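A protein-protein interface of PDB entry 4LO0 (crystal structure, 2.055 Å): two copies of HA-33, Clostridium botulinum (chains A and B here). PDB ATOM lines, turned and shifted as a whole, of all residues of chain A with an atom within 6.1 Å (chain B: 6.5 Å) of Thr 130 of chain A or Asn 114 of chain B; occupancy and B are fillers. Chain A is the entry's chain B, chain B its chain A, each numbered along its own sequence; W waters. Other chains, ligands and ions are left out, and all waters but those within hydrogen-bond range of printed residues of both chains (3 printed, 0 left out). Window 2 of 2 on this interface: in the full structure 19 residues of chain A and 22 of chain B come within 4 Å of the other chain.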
ATOM      1  N   ASN A 114      28.151  -2.917  22.227  1.00  0.00           N
ATOM      2  CA  ASN A 114      28.712  -1.560  22.109  1.00  0.00           C
ATOM      3  C   ASN A 114      28.293  -0.817  20.843  1.00  0.00           C
ATOM      4  O   ASN A 114      28.436   0.408  20.756  1.00  0.00           O
ATOM      5  CB  ASN A 114      30.242  -1.590  22.174  1.00  0.00           C
ATOM      6  CG  ASN A 114      30.737  -2.143  23.492  1.00  0.00           C
ATOM      7  OD1 ASN A 114      30.614  -1.489  24.535  1.00  0.00           O
ATOM      8  ND2 ASN A 114      31.287  -3.351  23.463  1.00  0.00           N
ATOM      9  N   LEU A 115      27.797  -1.553  19.856  1.00  0.00           N
ATOM     10  CA  LEU A 115      27.450  -0.934  18.575  1.00  0.00           C
ATOM     11  C   LEU A 115      25.945  -0.932  18.356  1.00  0.00           C
ATOM     12  O   LEU A 115      25.272  -1.946  18.569  1.00  0.00           O
ATOM     13  CB  LEU A 115      28.122  -1.689  17.415  1.00  0.00           C
ATOM     14  CG  LEU A 115      29.654  -1.649  17.472  1.00  0.00           C
ATOM     15  CD1 LEU A 115      30.256  -2.522  16.322  1.00  0.00           C
ATOM     16  CD2 LEU A 115      30.146  -0.181  17.361  1.00  0.00           C
ATOM     17  N   VAL A 116      25.422   0.208  17.919  1.00  0.00           N
ATOM     18  CA  VAL A 116      23.984   0.349  17.702  1.00  0.00           C
ATOM     19  C   VAL A 116      23.727   0.925  16.307  1.00  0.00           C
ATOM     20  O   VAL A 116      24.619   1.537  15.705  1.00  0.00           O
ATOM     21  CB  VAL A 116      23.350   1.262  18.773  1.00  0.00           C
ATOM     22  CG1 VAL A 116      23.785   0.810  20.186  1.00  0.00           C
ATOM     23  CG2 VAL A 116      23.778   2.725  18.526  1.00  0.00           C
ATOM     24  N   LEU A 128      26.680   1.892  11.807  1.00  0.00           N
ATOM     25  CA  LEU A 128      26.757   1.566  13.231  1.00  0.00           C
ATOM     26  C   LEU A 128      27.508   2.646  13.959  1.00  0.00           C
ATOM     27  O   LEU A 128      28.252   3.413  13.358  1.00  0.00           O
ATOM     28  CB  LEU A 128      27.449   0.221  13.471  1.00  0.00           C
ATOM     29  CG  LEU A 128      26.646  -1.012  13.060  1.00  0.00           C
ATOM     30  CD1 LEU A 128      27.514  -2.220  13.201  1.00  0.00           C
ATOM     31  CD2 LEU A 128      25.396  -1.173  13.951  1.00  0.00           C
ATOM     32  N   SER A 129      27.303   2.713  15.270  1.00  0.00           N
ATOM     33  CA  SER A 129      27.997   3.699  16.083  1.00  0.00           C
ATOM     34  C   SER A 129      28.059   3.150  17.476  1.00  0.00           C
ATOM     35  O   SER A 129      27.222   2.333  17.875  1.00  0.00           O
ATOM     36  CB  SER A 129      27.220   5.010  16.069  1.00  0.00           C
ATOM     37  OG  SER A 129      27.797   5.984  16.915  1.00  0.00           O
ATOM     38  N   THR A 130      29.055   3.591  18.227  1.00  0.00           N
ATOM     39  CA  THR A 130      28.985   3.395  19.654  1.00  0.00           C
ATOM     40  C   THR A 130      27.900   4.339  20.176  1.00  0.00           C
ATOM     41  O   THR A 130      27.424   5.225  19.445  1.00  0.00           O
ATOM     42  CB  THR A 130      30.348   3.624  20.346  1.00  0.00           C
ATOM     43  OG1 THR A 130      30.898   4.871  19.914  1.00  0.00           O
ATOM     44  CG2 THR A 130      31.301   2.505  19.993  1.00  0.00           C
ATOM     45  N   LEU A 131      27.487   4.126  21.423  1.00  0.00           N
ATOM     46  CA  LEU A 131      26.380   4.888  22.008  1.00  0.00           C
ATOM     47  C   LEU A 131      26.760   6.334  22.235  1.00  0.00           C
ATOM     48  O   LEU A 131      27.853   6.632  22.699  1.00  0.00           O
ATOM     49  CB  LEU A 131      26.033   4.344  23.386  1.00  0.00           C
ATOM     50  CG  LEU A 131      24.922   3.352  23.620  1.00  0.00           C
ATOM     51  CD1 LEU A 131      23.628   3.872  22.998  1.00  0.00           C
ATOM     52  CD2 LEU A 131      25.353   2.041  23.032  1.00  0.00           C
ATOM     53  N   ASN A 132      25.824   7.232  21.968  1.00  0.00           N
ATOM     54  CA  ASN A 132      26.042   8.642  22.215  1.00  0.00           C
ATOM     55  C   ASN A 132      24.666   9.226  22.399  1.00  0.00           C
ATOM     56  O   ASN A 132      23.686   8.493  22.454  1.00  0.00           O
ATOM     57  CB  ASN A 132      26.742   9.301  21.018  1.00  0.00           C
ATOM     58  CG  ASN A 132      26.010   9.029  19.700  1.00  0.00           C
ATOM     59  OD1 ASN A 132      24.838   9.384  19.535  1.00  0.00           O
ATOM     60  ND2 ASN A 132      26.700   8.391  18.764  1.00  0.00           N
ATOM     61  N   ILE A 137      20.830   7.695  16.379  1.00  0.00           N
ATOM     62  CA  ILE A 137      20.751   6.317  16.884  1.00  0.00           C
ATOM     63  C   ILE A 137      19.427   6.007  17.560  1.00  0.00           C
ATOM     64  O   ILE A 137      19.252   4.935  18.161  1.00  0.00           O
ATOM     65  CB  ILE A 137      21.902   5.968  17.870  1.00  0.00           C
ATOM     66  CG1 ILE A 137      21.743   6.754  19.168  1.00  0.00           C
ATOM     67  CG2 ILE A 137      23.257   6.238  17.217  1.00  0.00           C
ATOM     68  CD1 ILE A 137      22.671   6.275  20.289  1.00  0.00           C
ATOM     69  N   ALA B 108      22.799   4.156  31.364  1.00  0.00           N
ATOM     70  CA  ALA B 108      23.979   4.682  30.679  1.00  0.00           C
ATOM     71  C   ALA B 108      24.299   6.091  31.131  1.00  0.00           C
ATOM     72  O   ALA B 108      23.401   6.899  31.347  1.00  0.00           O
ATOM     73  CB  ALA B 108      23.751   4.685  29.190  1.00  0.00           C
ATOM     74  N   SER B 109      25.585   6.414  31.212  1.00  0.00           N
ATOM     75  CA  SER B 109      25.964   7.765  31.589  1.00  0.00           C
ATOM     76  C   SER B 109      25.581   8.748  30.494  1.00  0.00           C
ATOM     77  O   SER B 109      25.925   8.545  29.333  1.00  0.00           O
ATOM     78  CB  SER B 109      27.483   7.854  31.833  1.00  0.00           C
ATOM     79  OG  SER B 109      27.836   9.212  32.015  1.00  0.00           O
ATOM     80  N   ASN B 112      28.752  10.325  29.095  1.00  0.00           N
ATOM     81  CA  ASN B 112      29.429   9.479  28.113  1.00  0.00           C
ATOM     82  C   ASN B 112      28.684   8.164  27.943  1.00  0.00           C
ATOM     83  O   ASN B 112      28.974   7.189  28.644  1.00  0.00           O
ATOM     84  CB  ASN B 112      30.881   9.190  28.533  1.00  0.00           C
ATOM     85  CG  ASN B 112      31.665   8.468  27.430  1.00  0.00           C
ATOM     86  OD1 ASN B 112      31.067   7.779  26.584  1.00  0.00           O
ATOM     87  ND2 ASN B 112      33.004   8.634  27.422  1.00  0.00           N
ATOM     88  N   PRO B 113      27.745   8.111  26.982  1.00  0.00           N
ATOM     89  CA  PRO B 113      26.914   6.900  26.863  1.00  0.00           C
ATOM     90  C   PRO B 113      27.666   5.645  26.419  1.00  0.00           C
ATOM     91  O   PRO B 113      27.054   4.561  26.396  1.00  0.00           O
ATOM     92  CB  PRO B 113      25.832   7.303  25.843  1.00  0.00           C
ATOM     93  CG  PRO B 113      25.781   8.801  25.961  1.00  0.00           C
ATOM     94  CD  PRO B 113      27.211   9.232  26.196  1.00  0.00           C
ATOM     95  N   ASN B 114      28.949   5.762  26.065  1.00  0.00           N
ATOM     96  CA  ASN B 114      29.762   4.559  25.874  1.00  0.00           C
ATOM     97  C   ASN B 114      29.789   3.697  27.147  1.00  0.00           C
ATOM     98  O   ASN B 114      30.114   2.509  27.091  1.00  0.00           O
ATOM     99  CB  ASN B 114      31.231   4.916  25.571  1.00  0.00           C
ATOM    100  CG  ASN B 114      31.455   5.512  24.175  1.00  0.00           C
ATOM    101  OD1 ASN B 114      32.595   5.778  23.827  1.00  0.00           O
ATOM    102  ND2 ASN B 114      30.394   5.713  23.385  1.00  0.00           N
ATOM    103  N   LEU B 115      29.507   4.311  28.296  1.00  0.00           N
ATOM    104  CA  LEU B 115      29.684   3.646  29.592  1.00  0.00           C
ATOM    105  C   LEU B 115      28.348   3.494  30.313  1.00  0.00           C
ATOM    106  O   LEU B 115      27.534   4.404  30.284  1.00  0.00           O
ATOM    107  CB  LEU B 115      30.642   4.458  30.479  1.00  0.00           C
ATOM    108  CG  LEU B 115      32.045   4.597  29.883  1.00  0.00           C
ATOM    109  CD1 LEU B 115      32.815   5.702  30.641  1.00  0.00           C
ATOM    110  CD2 LEU B 115      32.750   3.272  30.009  1.00  0.00           C
ATOM    111  N   VAL B 116      28.148   2.346  30.966  1.00  0.00           N
ATOM    112  CA  VAL B 116      26.904   2.044  31.648  1.00  0.00           C
ATOM    113  C   VAL B 116      27.236   1.484  33.028  1.00  0.00           C
ATOM    114  O   VAL B 116      28.350   0.988  33.256  1.00  0.00           O
ATOM    115  CB  VAL B 116      26.042   1.008  30.848  1.00  0.00           C
ATOM    116  CG1 VAL B 116      25.888   1.439  29.356  1.00  0.00           C
ATOM    117  CG2 VAL B 116      26.669  -0.356  30.908  1.00  0.00           C
ATOM    118  N   SER B 129      31.149   0.668  32.952  1.00  0.00           N
ATOM    119  CA  SER B 129      31.709  -0.359  32.097  1.00  0.00           C
ATOM    120  C   SER B 129      31.219  -0.126  30.679  1.00  0.00           C
ATOM    121  O   SER B 129      30.175   0.499  30.482  1.00  0.00           O
ATOM    122  CB  SER B 129      31.231  -1.731  32.579  1.00  0.00           C
ATOM    123  OG  SER B 129      31.537  -2.766  31.662  1.00  0.00           O
ATOM    124  N   THR B 130      31.955  -0.645  29.701  1.00  0.00           N
ATOM    125  CA  THR B 130      31.423  -0.702  28.350  1.00  0.00           C
ATOM    126  C   THR B 130      30.367  -1.813  28.305  1.00  0.00           C
ATOM    127  O   THR B 130      30.218  -2.593  29.252  1.00  0.00           O
ATOM    128  CB  THR B 130      32.519  -0.970  27.320  1.00  0.00           C
ATOM    129  OG1 THR B 130      33.267  -2.119  27.728  1.00  0.00           O
ATOM    130  CG2 THR B 130      33.452   0.250  27.191  1.00  0.00           C
ATOM    131  N   LEU B 131      29.641  -1.909  27.205  1.00  0.00           N
ATOM    132  CA  LEU B 131      28.477  -2.802  27.195  1.00  0.00           C
ATOM    133  C   LEU B 131      28.843  -4.248  26.925  1.00  0.00           C
ATOM    134  O   LEU B 131      29.899  -4.557  26.347  1.00  0.00           O
ATOM    135  CB  LEU B 131      27.448  -2.320  26.172  1.00  0.00           C
ATOM    136  CG  LEU B 131      26.714  -1.057  26.618  1.00  0.00           C
ATOM    137  CD1 LEU B 131      27.531   0.199  26.313  1.00  0.00           C
ATOM    138  CD2 LEU B 131      25.310  -0.963  25.988  1.00  0.00           C
HETATM  139  O   HOH W   1      32.493  -4.271  26.230  1.00  0.00           O
HETATM  140  O   HOH W   2      30.716   1.217  24.849  1.00  0.00           O
HETATM  141  O   HOH W   3      33.353   5.314  21.176  1.00  0.00           O
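Printed residues of chain B within 4 Å of Asn 114 of chain A: Thr 130 (3.4 Å) and Leu 131 (2.9 Å). Ser 129 of chain A touches none of the printed residues of chain B. Thr 130 of chain A touches just one residue of chain B: Asn 114. Of the printed residues of chain B, Leu 131 of chain A touches Pro 113 and Asn 114. Ser 109 of chain B touches none of the printed residues of chain A. Printed residues of chain A within 4 Å of Pro 113 of chain B: Leu 131 and Asn 132. Asn 114 of chain B touches just these residues of chain A: Thr 130 (3.6 Å) and Leu 131 (2.8 Å). Printed residues of chain A within 4 Å of Thr 130 of chain B: Asn 114 (3.4 Å). Of the printed residues of chain A, Leu 131 of chain B touches Asn 114 (2.9 Å).
Of the 10 printed residues of chain B, 4 touch a printed residue of chain A. Printed residues of chain B that touch a printed residue of chain A: Pro 113, Asn 114, Thr 130 and Leu 131. Among the printed residues, 6 pairs touch across the chains.
Water W1 lies within hydrogen-bond range of O of Leu 131 of chain B (2.6 Å), OG1 of Thr 130 of chain B (2.7 Å) and ND2 of Asn 114 of chain A (3.2 Å). Water W2 lies within hydrogen-bond range of the backbone carbonyl oxygen of Asn 114 of chain B (2.7 Å) and the side-chain amide oxygen of Asn 114 of chain A (2.7 Å). Water W3 lies within hydrogen-bond range of the side-chain hydroxyl of Thr 130 of chain A (2.8 Å) and the side-chain amide oxygen of Asn 114 of chain B (2.8 Å).
Among the printed residues, pairs that only touch across the chains: Asn 114 of chain A with Thr 130 of chain B (3.4 Å), Thr 130 of chain A with Asn 114 of chain B (3.6 Å), Leu 131 of chain A with Pro 113 of chain B (3.2 Å) and Asn 132 of chain A with Pro 113 of chain B (3.8 Å).
The backbone carbonyl oxygen (O) of Thr 130 of chain A is in hydrogen-bond range of the side-chain amide nitrogen (ND2) of Asn 132 of chain A, at 3.3 Å. OG of Ser 129 of chain A is in hydrogen-bond range of ND2 of Asn 132 of chain A. The side-chain amide oxygen (OD1) of Asn 112 of chain B sits at hydrogen-bond distance from the backbone NH (N) of Asn 114 of chain B.
Asn 114 of chain A touches Thr 130 of chain B, and with the chains exchanged Thr 130 of chain A touches Asn 114 of chain B. Asn 114 of chain A touches Leu 131 of chain B, and with the chains exchanged Leu 131 of chain A touches Asn 114 of chain B. Of the 6 pairs that touch across the chains among the printed residues, 4 have their exchanged pair printed and touching as well.
N of Leu 131 of chain B sits at hydrogen-bond distance from OD1 of Asn 114 of chain A (2.9 Å). ND2 of Asn 114 of chain B lies within hydrogen-bond range of O of Leu 131 of chain A, 2.8 Å away.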
